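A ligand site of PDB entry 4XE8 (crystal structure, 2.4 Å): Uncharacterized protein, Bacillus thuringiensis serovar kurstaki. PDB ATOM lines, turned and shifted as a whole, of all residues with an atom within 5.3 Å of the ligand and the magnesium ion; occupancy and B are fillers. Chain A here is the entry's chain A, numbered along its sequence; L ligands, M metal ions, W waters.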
ATOM      1  N   ASP A  16     -26.711  -7.233 -20.766  1.00  0.00           N
ATOM      2  CA  ASP A  16     -25.519  -7.067 -21.596  1.00  0.00           C
ATOM      3  C   ASP A  16     -25.064  -8.411 -22.162  1.00  0.00           C
ATOM      4  O   ASP A  16     -24.394  -9.188 -21.487  1.00  0.00           O
ATOM      5  CB  ASP A  16     -24.403  -6.416 -20.778  1.00  0.00           C
ATOM      6  CG  ASP A  16     -23.107  -6.255 -21.546  1.00  0.00           C
ATOM      7  OD1 ASP A  16     -23.143  -6.259 -22.794  1.00  0.00           O
ATOM      8  OD2 ASP A  16     -22.040  -6.147 -20.896  1.00  0.00           O
ATOM      9  N   ILE A  20     -19.203 -14.194 -25.279  1.00  0.00           N
ATOM     10  CA  ILE A  20     -18.606 -14.925 -24.171  1.00  0.00           C
ATOM     11  C   ILE A  20     -19.652 -15.216 -23.086  1.00  0.00           C
ATOM     12  O   ILE A  20     -19.897 -16.371 -22.743  1.00  0.00           O
ATOM     13  CB  ILE A  20     -17.427 -14.160 -23.537  1.00  0.00           C
ATOM     14  CG1 ILE A  20     -16.452 -13.705 -24.616  1.00  0.00           C
ATOM     15  CG2 ILE A  20     -16.727 -15.016 -22.499  1.00  0.00           C
ATOM     16  CD1 ILE A  20     -15.734 -14.829 -25.307  1.00  0.00           C
ATOM     17  N   LYS A  21     -20.250 -14.149 -22.554  1.00  0.00           N
ATOM     18  CA  LYS A  21     -21.220 -14.266 -21.477  1.00  0.00           C
ATOM     19  C   LYS A  21     -22.481 -13.460 -21.765  1.00  0.00           C
ATOM     20  O   LYS A  21     -22.461 -12.494 -22.527  1.00  0.00           O
ATOM     21  CB  LYS A  21     -20.617 -13.808 -20.149  1.00  0.00           C
ATOM     22  CG  LYS A  21     -19.185 -14.240 -19.899  1.00  0.00           C
ATOM     23  CD  LYS A  21     -18.727 -13.839 -18.500  1.00  0.00           C
ATOM     24  CE  LYS A  21     -18.156 -12.432 -18.480  1.00  0.00           C
ATOM     25  NZ  LYS A  21     -16.886 -12.335 -19.262  1.00  0.00           N
ATOM     26  N   LYS A  23     -24.727 -11.126 -19.564  1.00  0.00           N
ATOM     27  CA  LYS A  23     -24.644 -10.461 -18.268  1.00  0.00           C
ATOM     28  C   LYS A  23     -25.932  -9.727 -17.907  1.00  0.00           C
ATOM     29  O   LYS A  23     -26.579  -9.127 -18.756  1.00  0.00           O
ATOM     30  CB  LYS A  23     -23.462  -9.500 -18.238  1.00  0.00           C
ATOM     31  CG  LYS A  23     -22.106 -10.198 -18.363  1.00  0.00           C
ATOM     32  CD  LYS A  23     -20.946  -9.292 -17.984  1.00  0.00           C
ATOM     33  CE  LYS A  23     -20.487  -8.450 -19.154  1.00  0.00           C
ATOM     34  NZ  LYS A  23     -19.225  -7.719 -18.843  1.00  0.00           N
ATOM     35  N   ASP A 236     -15.216  -0.141 -23.526  1.00  0.00           N
ATOM     36  CA  ASP A 236     -15.599  -1.329 -22.774  1.00  0.00           C
ATOM     37  C   ASP A 236     -14.614  -2.454 -23.067  1.00  0.00           C
ATOM     38  O   ASP A 236     -14.706  -3.120 -24.101  1.00  0.00           O
ATOM     39  CB  ASP A 236     -17.022  -1.759 -23.129  1.00  0.00           C
ATOM     40  CG  ASP A 236     -17.658  -2.625 -22.063  1.00  0.00           C
ATOM     41  OD1 ASP A 236     -16.931  -3.166 -21.200  1.00  0.00           O
ATOM     42  OD2 ASP A 236     -18.898  -2.773 -22.072  1.00  0.00           O
ATOM     43  N   LEU A 237     -13.661  -2.663 -22.164  1.00  0.00           N
ATOM     44  CA  LEU A 237     -12.618  -3.667 -22.369  1.00  0.00           C
ATOM     45  C   LEU A 237     -13.104  -5.045 -21.935  1.00  0.00           C
ATOM     46  O   LEU A 237     -13.263  -5.310 -20.742  1.00  0.00           O
ATOM     47  CB  LEU A 237     -11.347  -3.281 -21.608  1.00  0.00           C
ATOM     48  CG  LEU A 237     -10.872  -1.831 -21.712  1.00  0.00           C
ATOM     49  CD1 LEU A 237      -9.501  -1.676 -21.071  1.00  0.00           C
ATOM     50  CD2 LEU A 237     -10.845  -1.341 -23.159  1.00  0.00           C
ATOM     51  N   GLY A 238     -13.338  -5.926 -22.909  1.00  0.00           N
ATOM     52  CA  GLY A 238     -13.933  -7.220 -22.627  1.00  0.00           C
ATOM     53  C   GLY A 238     -13.006  -8.418 -22.789  1.00  0.00           C
ATOM     54  O   GLY A 238     -11.799  -8.265 -22.959  1.00  0.00           O
ATOM     55  N   ALA A 239     -13.600  -9.607 -22.734  1.00  0.00           N
ATOM     56  CA  ALA A 239     -12.835 -10.854 -22.767  1.00  0.00           C
ATOM     57  C   ALA A 239     -12.294 -11.169 -24.154  1.00  0.00           C
ATOM     58  O   ALA A 239     -11.109 -11.468 -24.320  1.00  0.00           O
ATOM     59  CB  ALA A 239     -13.699 -12.004 -22.274  1.00  0.00           C
ATOM     60  N   GLY A 240     -13.162 -11.102 -25.162  1.00  0.00           N
ATOM     61  CA  GLY A 240     -12.749 -11.384 -26.529  1.00  0.00           C
ATOM     62  C   GLY A 240     -12.824 -10.154 -27.410  1.00  0.00           C
ATOM     63  O   GLY A 240     -12.432 -10.197 -28.585  1.00  0.00           O
ATOM     64  N   THR A 241     -13.345  -9.058 -26.868  1.00  0.00           N
ATOM     65  CA  THR A 241     -13.538  -7.832 -27.639  1.00  0.00           C
ATOM     66  C   THR A 241     -13.195  -6.575 -26.847  1.00  0.00           C
ATOM     67  O   THR A 241     -13.001  -6.608 -25.640  1.00  0.00           O
ATOM     68  CB  THR A 241     -15.003  -7.694 -28.119  1.00  0.00           C
ATOM     69  OG1 THR A 241     -15.880  -7.696 -26.983  1.00  0.00           O
ATOM     70  CG2 THR A 241     -15.390  -8.835 -29.058  1.00  0.00           C
ATOM     71  N   THR A 264      -9.040  -9.809 -23.427  1.00  0.00           N
ATOM     72  CA  THR A 264      -8.107 -10.274 -22.419  1.00  0.00           C
ATOM     73  C   THR A 264      -7.731 -11.732 -22.630  1.00  0.00           C
ATOM     74  O   THR A 264      -6.660 -12.175 -22.204  1.00  0.00           O
ATOM     75  CB  THR A 264      -8.684 -10.122 -21.002  1.00  0.00           C
ATOM     76  OG1 THR A 264      -9.914 -10.859 -20.912  1.00  0.00           O
ATOM     77  CG2 THR A 264      -8.964  -8.667 -20.687  1.00  0.00           C
ATOM     78  N   ASN A 265      -8.626 -12.470 -23.286  1.00  0.00           N
ATOM     79  CA  ASN A 265      -8.494 -13.924 -23.414  1.00  0.00           C
ATOM     80  C   ASN A 265      -7.170 -14.378 -24.004  1.00  0.00           C
ATOM     81  O   ASN A 265      -6.581 -15.353 -23.538  1.00  0.00           O
ATOM     82  CB  ASN A 265      -9.647 -14.468 -24.253  1.00  0.00           C
ATOM     83  CG  ASN A 265     -10.948 -14.538 -23.479  1.00  0.00           C
ATOM     84  OD1 ASN A 265     -10.977 -14.386 -22.263  1.00  0.00           O
ATOM     85  ND2 ASN A 265     -12.051 -14.769 -24.197  1.00  0.00           N
ATOM     86  N   ILE A 268      -4.629 -13.986 -21.430  1.00  0.00           N
ATOM     87  CA  ILE A 268      -4.854 -15.022 -20.427  1.00  0.00           C
ATOM     88  C   ILE A 268      -4.344 -16.368 -20.939  1.00  0.00           C
ATOM     89  O   ILE A 268      -3.690 -17.106 -20.193  1.00  0.00           O
ATOM     90  CB  ILE A 268      -6.351 -15.133 -20.069  1.00  0.00           C
ATOM     91  CG1 ILE A 268      -6.852 -13.851 -19.416  1.00  0.00           C
ATOM     92  CG2 ILE A 268      -6.599 -16.321 -19.156  1.00  0.00           C
ATOM     93  CD1 ILE A 268      -8.337 -13.830 -19.167  1.00  0.00           C
ATOM     94  N   GLU A 301     -12.115 -18.474 -16.606  1.00  0.00           N
ATOM     95  CA  GLU A 301     -12.839 -17.934 -15.460  1.00  0.00           C
ATOM     96  C   GLU A 301     -12.319 -18.539 -14.161  1.00  0.00           C
ATOM     97  O   GLU A 301     -12.194 -17.842 -13.157  1.00  0.00           O
ATOM     98  CB  GLU A 301     -14.340 -18.189 -15.604  1.00  0.00           C
ATOM     99  CG  GLU A 301     -15.074 -17.097 -16.366  1.00  0.00           C
ATOM    100  CD  GLU A 301     -14.937 -15.751 -15.699  1.00  0.00           C
ATOM    101  OE1 GLU A 301     -14.978 -15.693 -14.451  1.00  0.00           O
ATOM    102  OE2 GLU A 301     -14.772 -14.736 -16.420  1.00  0.00           O
ATOM    103  N   ILE A 304      -9.162 -16.775 -13.482  1.00  0.00           N
ATOM    104  CA  ILE A 304      -9.447 -15.416 -13.021  1.00  0.00           C
ATOM    105  C   ILE A 304     -10.029 -15.412 -11.610  1.00  0.00           C
ATOM    106  O   ILE A 304      -9.604 -14.627 -10.758  1.00  0.00           O
ATOM    107  CB  ILE A 304     -10.424 -14.697 -13.983  1.00  0.00           C
ATOM    108  CG1 ILE A 304      -9.752 -14.477 -15.345  1.00  0.00           C
ATOM    109  CG2 ILE A 304     -10.868 -13.375 -13.397  1.00  0.00           C
ATOM    110  CD1 ILE A 304      -8.485 -13.660 -15.276  1.00  0.00           C
ATOM    111  N   VAL A 308      -6.560 -14.779  -9.821  1.00  0.00           N
ATOM    112  CA  VAL A 308      -6.357 -13.367 -10.139  1.00  0.00           C
ATOM    113  C   VAL A 308      -7.210 -12.400  -9.312  1.00  0.00           C
ATOM    114  O   VAL A 308      -6.677 -11.459  -8.717  1.00  0.00           O
ATOM    115  CB  VAL A 308      -6.624 -13.097 -11.626  1.00  0.00           C
ATOM    116  CG1 VAL A 308      -6.608 -11.608 -11.915  1.00  0.00           C
ATOM    117  CG2 VAL A 308      -5.592 -13.822 -12.484  1.00  0.00           C
ATOM    118  N   MET A 309      -8.516 -12.623  -9.282  1.00  0.00           N
ATOM    119  CA  MET A 309      -9.446 -11.723  -8.588  1.00  0.00           C
ATOM    120  C   MET A 309      -9.056 -11.363  -7.137  1.00  0.00           C
ATOM    121  O   MET A 309      -9.137 -10.193  -6.769  1.00  0.00           O
ATOM    122  CB  MET A 309     -10.866 -12.310  -8.601  1.00  0.00           C
ATOM    123  CG  MET A 309     -11.639 -12.050  -9.879  1.00  0.00           C
ATOM    124  SD  MET A 309     -13.276 -12.811  -9.860  1.00  0.00           S
ATOM    125  CE  MET A 309     -13.955 -12.202 -11.407  1.00  0.00           C
ATOM    126  N   VAL A 312      -6.193  -8.808  -7.270  1.00  0.00           N
ATOM    127  CA  VAL A 312      -6.612  -7.528  -7.831  1.00  0.00           C
ATOM    128  C   VAL A 312      -7.392  -6.711  -6.804  1.00  0.00           C
ATOM    129  O   VAL A 312      -7.222  -5.493  -6.707  1.00  0.00           O
ATOM    130  CB  VAL A 312      -7.461  -7.714  -9.105  1.00  0.00           C
ATOM    131  CG1 VAL A 312      -8.054  -6.392  -9.568  1.00  0.00           C
ATOM    132  CG2 VAL A 312      -6.618  -8.324 -10.209  1.00  0.00           C
ATOM    133  N   GLY A 371     -15.251  -2.150 -18.106  1.00  0.00           N
ATOM    134  CA  GLY A 371     -15.157  -3.553 -18.439  1.00  0.00           C
ATOM    135  C   GLY A 371     -14.218  -4.298 -17.507  1.00  0.00           C
ATOM    136  O   GLY A 371     -13.518  -3.693 -16.690  1.00  0.00           O
ATOM    137  N   GLY A 372     -14.207  -5.626 -17.616  1.00  0.00           N
ATOM    138  CA  GLY A 372     -13.350  -6.443 -16.772  1.00  0.00           C
ATOM    139  C   GLY A 372     -11.880  -6.262 -17.060  1.00  0.00           C
ATOM    140  O   GLY A 372     -11.030  -6.539 -16.211  1.00  0.00           O
ATOM    141  N   GLY A 373     -11.567  -5.776 -18.265  1.00  0.00           N
ATOM    142  CA  GLY A 373     -10.189  -5.528 -18.661  1.00  0.00           C
ATOM    143  C   GLY A 373      -9.513  -4.493 -17.783  1.00  0.00           C
ATOM    144  O   GLY A 373      -8.294  -4.533 -17.587  1.00  0.00           O
ATOM    145  N   LEU A 375      -9.950  -4.313 -14.622  1.00  0.00           N
ATOM    146  CA  LEU A 375      -9.559  -5.056 -13.433  1.00  0.00           C
ATOM    147  C   LEU A 375      -8.410  -6.016 -13.709  1.00  0.00           C
ATOM    148  O   LEU A 375      -7.449  -6.082 -12.942  1.00  0.00           O
ATOM    149  CB  LEU A 375     -10.759  -5.813 -12.865  1.00  0.00           C
ATOM    150  CG  LEU A 375     -11.876  -4.913 -12.318  1.00  0.00           C
ATOM    151  CD1 LEU A 375     -13.140  -5.725 -12.079  1.00  0.00           C
ATOM    152  CD2 LEU A 375     -11.418  -4.226 -11.042  1.00  0.00           C
ATOM    153  N   PHE A 376      -8.499  -6.754 -14.811  1.00  0.00           N
ATOM    154  CA  PHE A 376      -7.463  -7.707 -15.186  1.00  0.00           C
ATOM    155  C   PHE A 376      -6.112  -7.024 -15.380  1.00  0.00           C
ATOM    156  O   PHE A 376      -5.075  -7.552 -14.977  1.00  0.00           O
ATOM    157  CB  PHE A 376      -7.859  -8.460 -16.465  1.00  0.00           C
ATOM    158  CG  PHE A 376      -6.739  -9.287 -17.052  1.00  0.00           C
ATOM    159  CD1 PHE A 376      -6.372 -10.484 -16.467  1.00  0.00           C
ATOM    160  CD2 PHE A 376      -6.075  -8.869 -18.195  1.00  0.00           C
ATOM    161  CE1 PHE A 376      -5.349 -11.242 -16.999  1.00  0.00           C
ATOM    162  CE2 PHE A 376      -5.057  -9.620 -18.731  1.00  0.00           C
ATOM    163  CZ  PHE A 376      -4.694 -10.814 -18.136  1.00  0.00           C
ATOM    164  N   GLN A 397     -14.467  -1.638  -8.530  1.00  0.00           N
ATOM    165  CA  GLN A 397     -14.708  -3.061  -8.311  1.00  0.00           C
ATOM    166  C   GLN A 397     -15.876  -3.566  -9.155  1.00  0.00           C
ATOM    167  O   GLN A 397     -16.009  -4.762  -9.409  1.00  0.00           O
ATOM    168  CB  GLN A 397     -14.980  -3.327  -6.830  1.00  0.00           C
ATOM    169  CG  GLN A 397     -14.801  -4.776  -6.401  1.00  0.00           C
ATOM    170  CD  GLN A 397     -13.377  -5.096  -5.997  1.00  0.00           C
ATOM    171  OE1 GLN A 397     -12.862  -4.571  -5.007  1.00  0.00           O
ATOM    172  NE2 GLN A 397     -12.722  -5.961  -6.760  1.00  0.00           N
ATOM    173  N   ALA A 400     -16.603  -4.445 -14.352  1.00  0.00           N
ATOM    174  CA  ALA A 400     -16.928  -5.519 -15.286  1.00  0.00           C
ATOM    175  C   ALA A 400     -18.396  -5.458 -15.714  1.00  0.00           C
ATOM    176  O   ALA A 400     -18.730  -5.785 -16.843  1.00  0.00           O
ATOM    177  CB  ALA A 400     -16.611  -6.876 -14.676  1.00  0.00           C
HETATM  178  P1  LIG L   1     -17.312  -9.544 -21.605  1.00  0.00           P
HETATM  179  O1  LIG L   1     -18.071 -10.802 -21.252  1.00  0.00           O
HETATM  180  O2  LIG L   1     -16.761  -9.521 -23.025  1.00  0.00           O
HETATM  181  O3  LIG L   1     -18.000  -8.268 -21.209  1.00  0.00           O
HETATM  182  P2  LIG L   1     -15.848  -8.790 -19.305  1.00  0.00           P
HETATM  183  O4  LIG L   1     -16.930  -9.179 -18.317  1.00  0.00           O
HETATM  184  O5  LIG L   1     -15.662  -7.333 -19.642  1.00  0.00           O
HETATM  185  O6  LIG L   1     -15.999  -9.617 -20.681  1.00  0.00           O
HETATM  186  O7  LIG L   1     -14.457  -9.377 -18.752  1.00  0.00           O
HETATM  187  C1  LIG L   1     -13.216  -8.952 -19.314  1.00  0.00           C
HETATM  188  C2  LIG L   1     -12.097  -9.743 -18.643  1.00  0.00           C
HETATM  189  O8  LIG L   1     -11.834  -9.206 -17.344  1.00  0.00           O
HETATM  190  C3  LIG L   1     -12.482 -11.198 -18.459  1.00  0.00           C
HETATM  191  O9  LIG L   1     -11.415 -12.010 -18.949  1.00  0.00           O
HETATM  192  C4  LIG L   1     -12.609 -11.392 -16.966  1.00  0.00           C
HETATM  193  O10 LIG L   1     -12.131 -12.679 -16.567  1.00  0.00           O
HETATM  194  C5  LIG L   1     -11.753 -10.271 -16.396  1.00  0.00           C
HETATM  195  N1  LIG L   1     -12.221  -9.820 -15.062  1.00  0.00           N
HETATM  196  C6  LIG L   1     -13.486  -9.532 -14.692  1.00  0.00           C
HETATM  197  N2  LIG L   1     -13.528  -9.160 -13.386  1.00  0.00           N
HETATM  198  C7  LIG L   1     -12.269  -9.207 -12.898  1.00  0.00           C
HETATM  199  C8  LIG L   1     -11.604  -8.946 -11.603  1.00  0.00           C
HETATM  200  N3  LIG L   1     -12.302  -8.528 -10.525  1.00  0.00           N
HETATM  201  N4  LIG L   1     -10.261  -9.121 -11.545  1.00  0.00           N
HETATM  202  C9  LIG L   1      -9.546  -9.532 -12.608  1.00  0.00           C
HETATM  203  N5  LIG L   1     -10.087  -9.796 -13.811  1.00  0.00           N
HETATM  204  C10 LIG L   1     -11.420  -9.651 -14.012  1.00  0.00           C
HETATM  205 MG    MG M   1     -18.879  -6.820 -22.332  1.00  0.00          MG
HETATM  206  O   HOH W   1     -14.582  -7.283  -8.515  1.00  0.00           O
HETATM  207  O   HOH W   2     -11.085  -8.562  -7.971  1.00  0.00           O
HETATM  208  O   HOH W   3     -16.547 -10.593 -16.034  1.00  0.00           O
HETATM  209  O   HOH W   4     -19.222  -5.099 -23.713  1.00  0.00           O
HETATM  210  O   HOH W   5     -20.746 -10.090 -22.335  1.00  0.00           O
HETATM  211  O   HOH W   6     -19.545  -5.501 -20.769  1.00  0.00           O
HETATM  212  O   HOH W   7     -11.789 -14.492 -19.750  1.00  0.00           O
HETATM  213  O   HOH W   8     -16.901  -5.911 -21.578  1.00  0.00           O
HETATM  214  O   HOH W   9     -20.540  -7.662 -23.171  1.00  0.00           O
HETATM  215  O   HOH W  10     -17.566  -7.485 -23.949  1.00  0.00           O
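The side-chain amino group (NZ) of Lys 23 is in salt-bridge range of an oxygen (O4) of the ligand, 2.8 Å away. OG1 of Thr 264 lies within hydrogen-bond range of O9 of the ligand, 2.7 Å away. The side-chain amino group (NZ) of Lys 21 is in salt-bridge range of an oxygen (O1) of the ligand (2.8 Å). The backbone NH (N) of Gly 372 sits at hydrogen-bond distance from an oxygen (O5) of the ligand, 3.0 Å away. The backbone NH (N) of Ala 239 sits at hydrogen-bond distance from an oxygen (O6) of the ligand, at 3.2 Å. An oxygen (O10) of the ligand is in hydrogen-bond range of the side-chain carboxylate (OE2) of Glu 301 (3.4 Å).
The side-chain carboxylate (OD2) of Asp 16 is in salt-bridge range of the side-chain amino group (NZ) of Lys 23. O of Ala 400 is in hydrogen-bond range of NZ of Lys 23. N of Thr 264 lies within hydrogen-bond range of O of Ala 239. The backbone carbonyl oxygen (O) of Gly 238 sits at hydrogen-bond distance from the backbone NH (N) of Thr 264, 3.2 Å away. The backbone NH of Gly 372 is in hydrogen-bond range of the backbone carbonyl oxygen of Leu 237 (3.3 Å). O of Ala 239 lies within hydrogen-bond range of N of Asn 265 (2.9 Å). The backbone carbonyl oxygen (O) of Ile 304 lies within hydrogen-bond range of the backbone NH (N) of Met 309. The backbone carbonyl oxygen of Leu 237 lies within hydrogen-bond range of the backbone NH of Gly 373, 3.0 Å away.
The backbone carbonyl oxygen of Leu 237 lies close to an oxygen (O5) of the ligand (3.3 Å). Merely in contact with the ligand: Gly 238 (3.5 Å), Ile 268 (3.6 Å), Ile 304 (3.2 Å), Val 308 (3.7 Å), Met 309 (3.6 Å), Val 312 (3.96 Å), Gly 371 (3.98 Å), Gly 373 (3.6 Å), Leu 375 (3.3 Å) and Phe 376 (3.6 Å). Hydrophobic or aromatic side chains within 4 Å of the ligand: Ala 239, Ile 268, Ile 304, Val 308, Met 309, Val 312, Leu 375 and Phe 376. Of the 25 residues printed, 17 come within 4 Å of the ligand.
Residues that only touch the magnesium ion: Asp 16 (3.5 Å) and Lys 23 (3.6 Å).
An oxygen (O3) of the ligand is bound to the magnesium ion, at 2.0 Å. The magnesium ion is bound by water W9 (2.0 Å). Water W6 binds the magnesium ion, at 2.2 Å. The magnesium ion is bound by water W10, at 2.2 Å. The magnesium ion is bound by water W4. The magnesium ion is bound by water W8, at 2.3 Å. The magnesium ion has six donor atoms within binding distance.
Water W6 lies within hydrogen-bond range of OD2 of Asp 16 (2.6 Å), NZ of Lys 23 (3.0 Å) and OD2 of Asp 236 (3.1 Å). Water W8 lies within hydrogen-bond range of O5 of the ligand (2.7 Å) and OD1 of Asp 236 (2.8 Å). Water W7 lies within hydrogen-bond range of an oxygen (O9) of the ligand and the side-chain amide oxygen of Asn 265. Water W2 lies within hydrogen-bond range of the backbone carbonyl oxygen (O) of Met 309 (2.8 Å), a nitrogen (N3) of the ligand (2.8 Å) and the side-chain amide nitrogen (NE2) of Gln 397 (3.3 Å). Water W5 bridges O of Lys 21 (3.0 Å) and O1 of the ligand (3.0 Å). Water W1 bridges NE2 of Gln 397 (2.9 Å) and N3 of the ligand (3.3 Å).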
